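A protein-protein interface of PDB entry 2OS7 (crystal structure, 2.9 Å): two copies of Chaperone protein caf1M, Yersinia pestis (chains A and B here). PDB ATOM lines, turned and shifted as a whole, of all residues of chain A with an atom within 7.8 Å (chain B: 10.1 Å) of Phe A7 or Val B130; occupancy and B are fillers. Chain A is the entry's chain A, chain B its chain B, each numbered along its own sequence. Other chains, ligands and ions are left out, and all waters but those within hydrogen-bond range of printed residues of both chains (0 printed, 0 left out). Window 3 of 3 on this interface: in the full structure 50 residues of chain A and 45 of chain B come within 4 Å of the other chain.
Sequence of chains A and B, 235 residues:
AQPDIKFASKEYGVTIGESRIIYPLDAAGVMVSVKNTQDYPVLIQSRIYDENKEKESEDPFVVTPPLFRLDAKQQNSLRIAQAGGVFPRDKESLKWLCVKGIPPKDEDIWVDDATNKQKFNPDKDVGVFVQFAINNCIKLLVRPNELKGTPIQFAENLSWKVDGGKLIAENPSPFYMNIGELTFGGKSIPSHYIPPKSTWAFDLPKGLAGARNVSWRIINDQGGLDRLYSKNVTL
The side-chain hydroxyl (OG1) of Thr B37 lies within hydrogen-bond range of the side-chain hydroxyl (OG) of Ser A9 (3.0 Å).
OH of Tyr A12 is in hydrogen-bond range of OE2 of Glu B11 (2.7 Å).
The backbone carbonyl oxygen (O) of Tyr A12 is in hydrogen-bond range of the side-chain amide nitrogen (NE2) of Gln B38, at 3.5 Å.
The backbone carbonyl oxygen of Val A130 sits at hydrogen-bond distance from the backbone NH of Lys B10 (3.1 Å).
The backbone NH (N) of Phe A132 lies within hydrogen-bond range of the backbone carbonyl oxygen (O) of Lys B10, at 2.9 Å.
CG2 of Val B130 touches CE1 of Phe A7, 3.8 Å away.
Phe A7 touches Phe B132.
Ala A8 touches Gln B38 (CB to NE2, 3.4 Å).
Ala A8 touches Phe B132 (CB to CZ, 3.8 Å).
Ser A9 touches Gln B38.
Phe B132 touches Tyr A12 (CE1 to O, 3.3 Å).
Val A130 touches Ser B9 (O to CA, 3.2 Å).
Lys B10 touches Gln A131.
Phe A132 touches Ser B9.
Glu B11 touches Phe A132.
Of chain B, only Val B130 and Phe B132 come within 4 Å of Phe A7.
Val B130 touches one residue of chain A.
Of chain B, only Gln B38 (3.4 Å) and Phe B132 (3.8 Å) come within 4 Å of Ala A8.
Of the printed residues of chain A, Lys B10 touches Val A130 (3.1 Å), Gln A131 (3.8 Å) and Phe A132 (2.9 Å).
Of the printed residues of chain A, Thr B37 touches Ser A9.
Of the printed residues of chain A, Glu B11 touches Tyr A12 (2.7 Å) and Phe A132 (3.5 Å).
Of the printed residues of chain A, Phe B132 touches Phe A7 (3.7 Å), Ala A8 (3.8 Å) and Tyr A12 (3.3 Å).
Of the printed residues of chain B, Tyr A12 touches Glu B11 (2.7 Å), Gln B38 (3.5 Å), Phe B132 (3.3 Å) and Ile B134 (3.8 Å).
Gly B127 touches none of the printed residues of chain A.
The nearest residue of chain B that does not touch Phe A7 is Gln B38 (4.9 Å).
The nearest residue of chain A that does not touch Val B130 is Phe A132 (6.8 Å).
Of the 11 printed residues of chain A, 7 touch a printed residue of chain B.
Hydrophobic or aromatic side chains of chain A within 4 Å of the printed part of chain B: Phe A7, Ala A8, Tyr A12, Val A130 and Phe A132.
Of the 17 printed residues of chain B, 8 touch a printed residue of chain A.
Printed residues of chain B that touch a printed residue of chain A: Ser B9, Lys B10, Glu B11, Thr B37, Gln B38, Val B130, Phe B132 and Ile B134.
Hydrophobic or aromatic side chains of chain B that line the printed part of chain A: Val B130, Phe B132 and Ile B134.
Among the printed residues, no Asp or Glu carboxylate lies within 4 Å of a Lys or Arg side-chain nitrogen of the other chain.
Phe A7 touches Val B130, but with the chains exchanged Val A130 does not touch Phe B7 (4.4 Å).
Phe A7 touches Phe B132, but with the chains exchanged Phe A132 does not touch Phe B7 (6.6 Å).
Val A130 touches Ser B9, but with the chains exchanged Ser A9 does not touch Val B130 (11.6 Å).
Phe A132 touches Ser B9, but with the chains exchanged Ser A9 does not touch Phe B132 (6.1 Å).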
ATOM      1  N   ASP A   4       8.852  -4.911  -1.578  1.00  0.00           N
ATOM      2  CA  ASP A   4       9.074  -3.501  -1.191  1.00  0.00           C
ATOM      3  C   ASP A   4       9.470  -2.643  -2.419  1.00  0.00           C
ATOM      4  O   ASP A   4      10.437  -2.962  -3.132  1.00  0.00           O
ATOM      5  CB  ASP A   4      10.156  -3.413  -0.101  1.00  0.00           C
ATOM      6  CG  ASP A   4       9.767  -4.156   1.179  1.00  0.00           C
ATOM      7  OD1 ASP A   4       9.412  -3.464   2.178  1.00  0.00           O
ATOM      8  OD2 ASP A   4       9.794  -5.421   1.177  1.00  0.00           O
ATOM      9  N   ILE A   5       8.735  -1.565  -2.678  1.00  0.00           N
ATOM     10  CA  ILE A   5       8.902  -0.841  -3.947  1.00  0.00           C
ATOM     11  C   ILE A   5      10.191  -0.007  -3.947  1.00  0.00           C
ATOM     12  O   ILE A   5      10.283   1.006  -3.258  1.00  0.00           O
ATOM     13  CB  ILE A   5       7.643   0.037  -4.338  1.00  0.00           C
ATOM     14  CG1 ILE A   5       6.326  -0.731  -4.157  1.00  0.00           C
ATOM     15  CG2 ILE A   5       7.804   0.658  -5.744  1.00  0.00           C
ATOM     16  CD1 ILE A   5       6.183  -1.993  -4.986  1.00  0.00           C
ATOM     17  N   LYS A   6      11.168  -0.442  -4.740  1.00  0.00           N
ATOM     18  CA  LYS A   6      12.500   0.154  -4.734  1.00  0.00           C
ATOM     19  C   LYS A   6      12.541   1.307  -5.665  1.00  0.00           C
ATOM     20  O   LYS A   6      12.173   1.188  -6.823  1.00  0.00           O
ATOM     21  CB  LYS A   6      13.599  -0.852  -5.099  1.00  0.00           C
ATOM     22  CG  LYS A   6      14.948  -0.219  -5.218  1.00  0.00           C
ATOM     23  CD  LYS A   6      16.014  -1.114  -4.665  1.00  0.00           C
ATOM     24  CE  LYS A   6      17.410  -0.648  -5.062  1.00  0.00           C
ATOM     25  NZ  LYS A   6      18.469  -1.569  -4.554  1.00  0.00           N
ATOM     26  N   PHE A   7      13.006   2.427  -5.146  1.00  0.00           N
ATOM     27  CA  PHE A   7      13.013   3.643  -5.895  1.00  0.00           C
ATOM     28  C   PHE A   7      14.381   3.956  -6.491  1.00  0.00           C
ATOM     29  O   PHE A   7      14.486   4.209  -7.689  1.00  0.00           O
ATOM     30  CB  PHE A   7      12.560   4.779  -5.009  1.00  0.00           C
ATOM     31  CG  PHE A   7      12.366   6.037  -5.741  1.00  0.00           C
ATOM     32  CD1 PHE A   7      11.283   6.169  -6.639  1.00  0.00           C
ATOM     33  CD2 PHE A   7      13.256   7.081  -5.579  1.00  0.00           C
ATOM     34  CE1 PHE A   7      11.093   7.360  -7.359  1.00  0.00           C
ATOM     35  CE2 PHE A   7      13.093   8.273  -6.281  1.00  0.00           C
ATOM     36  CZ  PHE A   7      12.010   8.429  -7.163  1.00  0.00           C
ATOM     37  N   ALA A   8      15.416   3.984  -5.652  1.00  0.00           N
ATOM     38  CA  ALA A   8      16.788   4.166  -6.108  1.00  0.00           C
ATOM     39  C   ALA A   8      17.642   3.193  -5.347  1.00  0.00           C
ATOM     40  O   ALA A   8      17.122   2.424  -4.575  1.00  0.00           O
ATOM     41  CB  ALA A   8      17.249   5.608  -5.912  1.00  0.00           C
ATOM     42  N   SER A   9      18.941   3.207  -5.617  1.00  0.00           N
ATOM     43  CA  SER A   9      19.951   2.376  -4.917  1.00  0.00           C
ATOM     44  C   SER A   9      20.891   3.303  -4.125  1.00  0.00           C
ATOM     45  O   SER A   9      20.601   4.494  -4.037  1.00  0.00           O
ATOM     46  CB  SER A   9      20.699   1.457  -5.919  1.00  0.00           C
ATOM     47  OG  SER A   9      20.824   2.030  -7.244  1.00  0.00           O
ATOM     48  N   TYR A  12      21.386   7.388  -3.465  1.00  0.00           N
ATOM     49  CA  TYR A  12      20.479   7.775  -4.633  1.00  0.00           C
ATOM     50  C   TYR A  12      20.998   7.547  -6.069  1.00  0.00           C
ATOM     51  O   TYR A  12      20.602   8.229  -7.025  1.00  0.00           O
ATOM     52  CB  TYR A  12      19.923   9.192  -4.493  1.00  0.00           C
ATOM     53  CG  TYR A  12      18.671   9.335  -3.643  1.00  0.00           C
ATOM     54  CD1 TYR A  12      18.760   9.761  -2.327  1.00  0.00           C
ATOM     55  CD2 TYR A  12      17.394   9.115  -4.179  1.00  0.00           C
ATOM     56  CE1 TYR A  12      17.653   9.937  -1.553  1.00  0.00           C
ATOM     57  CE2 TYR A  12      16.252   9.305  -3.397  1.00  0.00           C
ATOM     58  CZ  TYR A  12      16.399   9.715  -2.074  1.00  0.00           C
ATOM     59  OH  TYR A  12      15.299   9.893  -1.250  1.00  0.00           O
ATOM     60  N   VAL A 130       3.639  11.162   0.023  1.00  0.00           N
ATOM     61  CA  VAL A 130       4.670  10.180  -0.274  1.00  0.00           C
ATOM     62  C   VAL A 130       5.686  10.045   0.854  1.00  0.00           C
ATOM     63  O   VAL A 130       6.128  11.032   1.459  1.00  0.00           O
ATOM     64  CB  VAL A 130       5.421  10.524  -1.564  1.00  0.00           C
ATOM     65  CG1 VAL A 130       6.303   9.396  -1.984  1.00  0.00           C
ATOM     66  CG2 VAL A 130       4.451  10.809  -2.683  1.00  0.00           C
ATOM     67  N   GLN A 131       6.056   8.798   1.118  1.00  0.00           N
ATOM     68  CA  GLN A 131       7.056   8.479   2.098  1.00  0.00           C
ATOM     69  C   GLN A 131       8.203   7.686   1.485  1.00  0.00           C
ATOM     70  O   GLN A 131       8.007   6.573   0.975  1.00  0.00           O
ATOM     71  CB  GLN A 131       6.431   7.732   3.260  1.00  0.00           C
ATOM     72  CG  GLN A 131       5.562   8.636   4.120  1.00  0.00           C
ATOM     73  CD  GLN A 131       4.936   7.901   5.302  1.00  0.00           C
ATOM     74  OE1 GLN A 131       4.988   6.642   5.374  1.00  0.00           O
ATOM     75  NE2 GLN A 131       4.338   8.676   6.245  1.00  0.00           N
ATOM     76  N   PHE A 132       9.394   8.302   1.538  1.00  0.00           N
ATOM     77  CA  PHE A 132      10.677   7.714   1.110  1.00  0.00           C
ATOM     78  C   PHE A 132      11.438   7.135   2.294  1.00  0.00           C
ATOM     79  O   PHE A 132      11.761   7.848   3.274  1.00  0.00           O
ATOM     80  CB  PHE A 132      11.550   8.750   0.416  1.00  0.00           C
ATOM     81  CG  PHE A 132      10.962   9.283  -0.843  1.00  0.00           C
ATOM     82  CD1 PHE A 132      10.015  10.288  -0.817  1.00  0.00           C
ATOM     83  CD2 PHE A 132      11.355   8.783  -2.068  1.00  0.00           C
ATOM     84  CE1 PHE A 132       9.463  10.786  -2.004  1.00  0.00           C
ATOM     85  CE2 PHE A 132      10.793   9.264  -3.266  1.00  0.00           C
ATOM     86  CZ  PHE A 132       9.854  10.263  -3.230  1.00  0.00           C
ATOM     87  N   ALA A 133      11.723   5.839   2.207  1.00  0.00           N
ATOM     88  CA  ALA A 133      12.361   5.111   3.306  1.00  0.00           C
ATOM     89  C   ALA A 133      13.755   4.651   2.910  1.00  0.00           C
ATOM     90  O   ALA A 133      13.884   3.736   2.106  1.00  0.00           O
ATOM     91  CB  ALA A 133      11.500   3.936   3.731  1.00  0.00           C
ATOM     92  N   PHE B   7       0.388  17.799  -2.547  1.00  0.00           N
ATOM     93  CA  PHE B   7       1.398  16.814  -2.867  1.00  0.00           C
ATOM     94  C   PHE B   7       2.565  17.071  -1.921  1.00  0.00           C
ATOM     95  O   PHE B   7       3.106  18.183  -1.849  1.00  0.00           O
ATOM     96  CB  PHE B   7       1.840  16.958  -4.326  1.00  0.00           C
ATOM     97  CG  PHE B   7       2.916  15.986  -4.730  1.00  0.00           C
ATOM     98  CD1 PHE B   7       2.595  14.814  -5.414  1.00  0.00           C
ATOM     99  CD2 PHE B   7       4.247  16.224  -4.415  1.00  0.00           C
ATOM    100  CE1 PHE B   7       3.580  13.894  -5.779  1.00  0.00           C
ATOM    101  CE2 PHE B   7       5.240  15.309  -4.776  1.00  0.00           C
ATOM    102  CZ  PHE B   7       4.905  14.138  -5.457  1.00  0.00           C
ATOM    103  N   SER B   9       6.024  15.122   0.351  1.00  0.00           N
ATOM    104  CA  SER B   9       6.906  13.977   0.541  1.00  0.00           C
ATOM    105  C   SER B   9       7.906  14.242   1.631  1.00  0.00           C
ATOM    106  O   SER B   9       8.353  15.370   1.809  1.00  0.00           O
ATOM    107  CB  SER B   9       7.619  13.593  -0.762  1.00  0.00           C
ATOM    108  OG  SER B   9       8.400  14.663  -1.260  1.00  0.00           O
ATOM    109  N   LYS B  10       8.220  13.190   2.379  1.00  0.00           N
ATOM    110  CA  LYS B  10       9.287  13.223   3.368  1.00  0.00           C
ATOM    111  C   LYS B  10      10.222  12.042   3.109  1.00  0.00           C
ATOM    112  O   LYS B  10       9.822  11.028   2.533  1.00  0.00           O
ATOM    113  CB  LYS B  10       8.725  13.152   4.786  1.00  0.00           C
ATOM    114  CG  LYS B  10       8.278  14.472   5.399  1.00  0.00           C
ATOM    115  CD  LYS B  10       7.824  14.243   6.868  1.00  0.00           C
ATOM    116  CE  LYS B  10       6.749  15.226   7.312  1.00  0.00           C
ATOM    117  NZ  LYS B  10       6.409  15.034   8.756  1.00  0.00           N
ATOM    118  N   GLU B  11      11.458  12.207   3.574  1.00  0.00           N
ATOM    119  CA  GLU B  11      12.552  11.278   3.403  1.00  0.00           C
ATOM    120  C   GLU B  11      12.979  10.860   4.795  1.00  0.00           C
ATOM    121  O   GLU B  11      13.119  11.721   5.668  1.00  0.00           O
ATOM    122  CB  GLU B  11      13.665  12.070   2.752  1.00  0.00           C
ATOM    123  CG  GLU B  11      14.864  11.309   2.276  1.00  0.00           C
ATOM    124  CD  GLU B  11      15.768  12.161   1.431  1.00  0.00           C
ATOM    125  OE1 GLU B  11      15.912  13.366   1.709  1.00  0.00           O
ATOM    126  OE2 GLU B  11      16.327  11.630   0.470  1.00  0.00           O
ATOM    127  N   THR B  37      24.935   3.623  -9.711  1.00  0.00           N
ATOM    128  CA  THR B  37      24.350   2.354  -9.289  1.00  0.00           C
ATOM    129  C   THR B  37      22.946   2.166  -9.781  1.00  0.00           C
ATOM    130  O   THR B  37      22.400   1.071  -9.647  1.00  0.00           O
ATOM    131  CB  THR B  37      24.335   2.186  -7.781  1.00  0.00           C
ATOM    132  OG1 THR B  37      23.567   3.243  -7.216  1.00  0.00           O
ATOM    133  CG2 THR B  37      25.741   2.244  -7.217  1.00  0.00           C
ATOM    134  N   GLN B  38      22.341   3.212 -10.339  1.00  0.00           N
ATOM    135  CA  GLN B  38      21.147   3.040 -11.163  1.00  0.00           C
ATOM    136  C   GLN B  38      21.451   2.080 -12.292  1.00  0.00           C
ATOM    137  O   GLN B  38      22.595   1.773 -12.562  1.00  0.00           O
ATOM    138  CB  GLN B  38      20.707   4.371 -11.763  1.00  0.00           C
ATOM    139  CG  GLN B  38      20.187   5.362 -10.762  1.00  0.00           C
ATOM    140  CD  GLN B  38      19.396   4.718  -9.663  1.00  0.00           C
ATOM    141  OE1 GLN B  38      18.870   3.631  -9.813  1.00  0.00           O
ATOM    142  NE2 GLN B  38      19.315   5.385  -8.543  1.00  0.00           N
ATOM    143  N   ASP B  39      20.430   1.610 -12.981  1.00  0.00           N
ATOM    144  CA  ASP B  39      20.664   0.721 -14.128  1.00  0.00           C
ATOM    145  C   ASP B  39      20.435   1.444 -15.442  1.00  0.00           C
ATOM    146  O   ASP B  39      20.181   0.783 -16.448  1.00  0.00           O
ATOM    147  CB  ASP B  39      19.727  -0.470 -14.062  1.00  0.00           C
ATOM    148  CG  ASP B  39      18.298  -0.023 -13.996  1.00  0.00           C
ATOM    149  OD1 ASP B  39      18.045   1.088 -14.546  1.00  0.00           O
ATOM    150  OD2 ASP B  39      17.455  -0.733 -13.370  1.00  0.00           O
ATOM    151  N   TYR B  40      20.509   2.780 -15.417  1.00  0.00           N
ATOM    152  CA  TYR B  40      20.469   3.614 -16.632  1.00  0.00           C
ATOM    153  C   TYR B  40      21.640   4.601 -16.660  1.00  0.00           C
ATOM    154  O   TYR B  40      22.234   4.860 -15.621  1.00  0.00           O
ATOM    155  CB  TYR B  40      19.134   4.359 -16.755  1.00  0.00           C
ATOM    156  CG  TYR B  40      18.806   5.205 -15.562  1.00  0.00           C
ATOM    157  CD1 TYR B  40      19.406   6.464 -15.382  1.00  0.00           C
ATOM    158  CD2 TYR B  40      17.901   4.759 -14.595  1.00  0.00           C
ATOM    159  CE1 TYR B  40      19.126   7.266 -14.231  1.00  0.00           C
ATOM    160  CE2 TYR B  40      17.592   5.553 -13.439  1.00  0.00           C
ATOM    161  CZ  TYR B  40      18.211   6.800 -13.265  1.00  0.00           C
ATOM    162  OH  TYR B  40      17.914   7.570 -12.157  1.00  0.00           O
ATOM    163  N   PRO B 103      20.057  12.819 -15.369  1.00  0.00           N
ATOM    164  CA  PRO B 103      19.781  11.910 -16.471  1.00  0.00           C
ATOM    165  C   PRO B 103      19.428  12.633 -17.746  1.00  0.00           C
ATOM    166  O   PRO B 103      19.227  11.957 -18.746  1.00  0.00           O
ATOM    167  CB  PRO B 103      18.608  11.105 -15.950  1.00  0.00           C
ATOM    168  CG  PRO B 103      17.977  11.967 -14.846  1.00  0.00           C
ATOM    169  CD  PRO B 103      18.816  13.198 -14.670  1.00  0.00           C
ATOM    170  N   GLY B 127      -0.248   6.899 -16.431  1.00  0.00           N
ATOM    171  CA  GLY B 127       0.116   6.999 -15.042  1.00  0.00           C
ATOM    172  C   GLY B 127       1.154   8.042 -14.719  1.00  0.00           C
ATOM    173  O   GLY B 127       1.340   8.990 -15.464  1.00  0.00           O
ATOM    174  N   VAL B 128       1.830   7.855 -13.593  1.00  0.00           N
ATOM    175  CA  VAL B 128       2.837   8.783 -13.104  1.00  0.00           C
ATOM    176  C   VAL B 128       4.201   8.205 -13.388  1.00  0.00           C
ATOM    177  O   VAL B 128       4.456   7.064 -13.046  1.00  0.00           O
ATOM    178  CB  VAL B 128       2.657   9.010 -11.591  1.00  0.00           C
ATOM    179  CG1 VAL B 128       3.433  10.210 -11.120  1.00  0.00           C
ATOM    180  CG2 VAL B 128       1.178   9.197 -11.281  1.00  0.00           C
ATOM    181  N   PHE B 129       5.060   8.990 -14.047  1.00  0.00           N
ATOM    182  CA  PHE B 129       6.459   8.593 -14.341  1.00  0.00           C
ATOM    183  C   PHE B 129       7.431   9.535 -13.649  1.00  0.00           C
ATOM    184  O   PHE B 129       7.121  10.718 -13.511  1.00  0.00           O
ATOM    185  CB  PHE B 129       6.723   8.563 -15.837  1.00  0.00           C
ATOM    186  CG  PHE B 129       5.856   7.597 -16.592  1.00  0.00           C
ATOM    187  CD1 PHE B 129       4.556   7.945 -16.978  1.00  0.00           C
ATOM    188  CD2 PHE B 129       6.339   6.343 -16.943  1.00  0.00           C
ATOM    189  CE1 PHE B 129       3.765   7.050 -17.683  1.00  0.00           C
ATOM    190  CE2 PHE B 129       5.547   5.447 -17.661  1.00  0.00           C
ATOM    191  CZ  PHE B 129       4.250   5.808 -18.027  1.00  0.00           C
ATOM    192  N   VAL B 130       8.585   9.022 -13.195  1.00  0.00           N
ATOM    193  CA  VAL B 130       9.539   9.851 -12.409  1.00  0.00           C
ATOM    194  C   VAL B 130      10.916   9.952 -12.944  1.00  0.00           C
ATOM    195  O   VAL B 130      11.417   9.031 -13.582  1.00  0.00           O
ATOM    196  CB  VAL B 130       9.787   9.355 -10.969  1.00  0.00           C
ATOM    197  CG1 VAL B 130       8.936  10.132 -10.000  1.00  0.00           C
ATOM    198  CG2 VAL B 130       9.636   7.841 -10.862  1.00  0.00           C
ATOM    199  N   GLN B 131      11.535  11.074 -12.602  1.00  0.00           N
ATOM    200  CA  GLN B 131      12.951  11.306 -12.810  1.00  0.00           C
ATOM    201  C   GLN B 131      13.511  12.059 -11.606  1.00  0.00           C
ATOM    202  O   GLN B 131      12.782  12.768 -10.906  1.00  0.00           O
ATOM    203  CB  GLN B 131      13.146  12.107 -14.073  1.00  0.00           C
ATOM    204  CG  GLN B 131      13.173  11.239 -15.276  1.00  0.00           C
ATOM    205  CD  GLN B 131      13.534  12.006 -16.497  1.00  0.00           C
ATOM    206  OE1 GLN B 131      13.132  13.166 -16.642  1.00  0.00           O
ATOM    207  NE2 GLN B 131      14.304  11.374 -17.397  1.00  0.00           N
ATOM    208  N   PHE B 132      14.795  11.886 -11.338  1.00  0.00           N
ATOM    209  CA  PHE B 132      15.400  12.676 -10.279  1.00  0.00           C
ATOM    210  C   PHE B 132      16.837  12.968 -10.595  1.00  0.00           C
ATOM    211  O   PHE B 132      17.511  12.163 -11.241  1.00  0.00           O
ATOM    212  CB  PHE B 132      15.258  12.010  -8.905  1.00  0.00           C
ATOM    213  CG  PHE B 132      15.832  10.636  -8.848  1.00  0.00           C
ATOM    214  CD1 PHE B 132      17.169  10.443  -8.523  1.00  0.00           C
ATOM    215  CD2 PHE B 132      15.042   9.533  -9.129  1.00  0.00           C
ATOM    216  CE1 PHE B 132      17.731   9.149  -8.482  1.00  0.00           C
ATOM    217  CE2 PHE B 132      15.580   8.260  -9.103  1.00  0.00           C
ATOM    218  CZ  PHE B 132      16.952   8.057  -8.787  1.00  0.00           C
ATOM    219  N   ALA B 133      17.268  14.150 -10.167  1.00  0.00           N
ATOM    220  CA  ALA B 133      18.663  14.550 -10.179  1.00  0.00           C
ATOM    221  C   ALA B 133      19.198  14.446  -8.748  1.00  0.00           C
ATOM    222  O   ALA B 133      18.450  14.637  -7.775  1.00  0.00           O
ATOM    223  CB  ALA B 133      18.785  15.945 -10.700  1.00  0.00           C
ATOM    224  N   ILE B 134      20.478  14.116  -8.620  1.00  0.00           N
ATOM    225  CA  ILE B 134      21.082  13.895  -7.291  1.00  0.00           C
ATOM    226  C   ILE B 134      22.356  14.637  -7.157  1.00  0.00           C
ATOM    227  O   ILE B 134      23.210  14.583  -8.037  1.00  0.00           O
ATOM    228  CB  ILE B 134      21.378  12.413  -6.977  1.00  0.00           C
ATOM    229  CG1 ILE B 134      22.098  12.303  -5.658  1.00  0.00           C
ATOM    230  CG2 ILE B 134      22.223  11.754  -8.047  1.00  0.00           C
ATOM    231  CD1 ILE B 134      21.272  12.796  -4.463  1.00  0.00           C
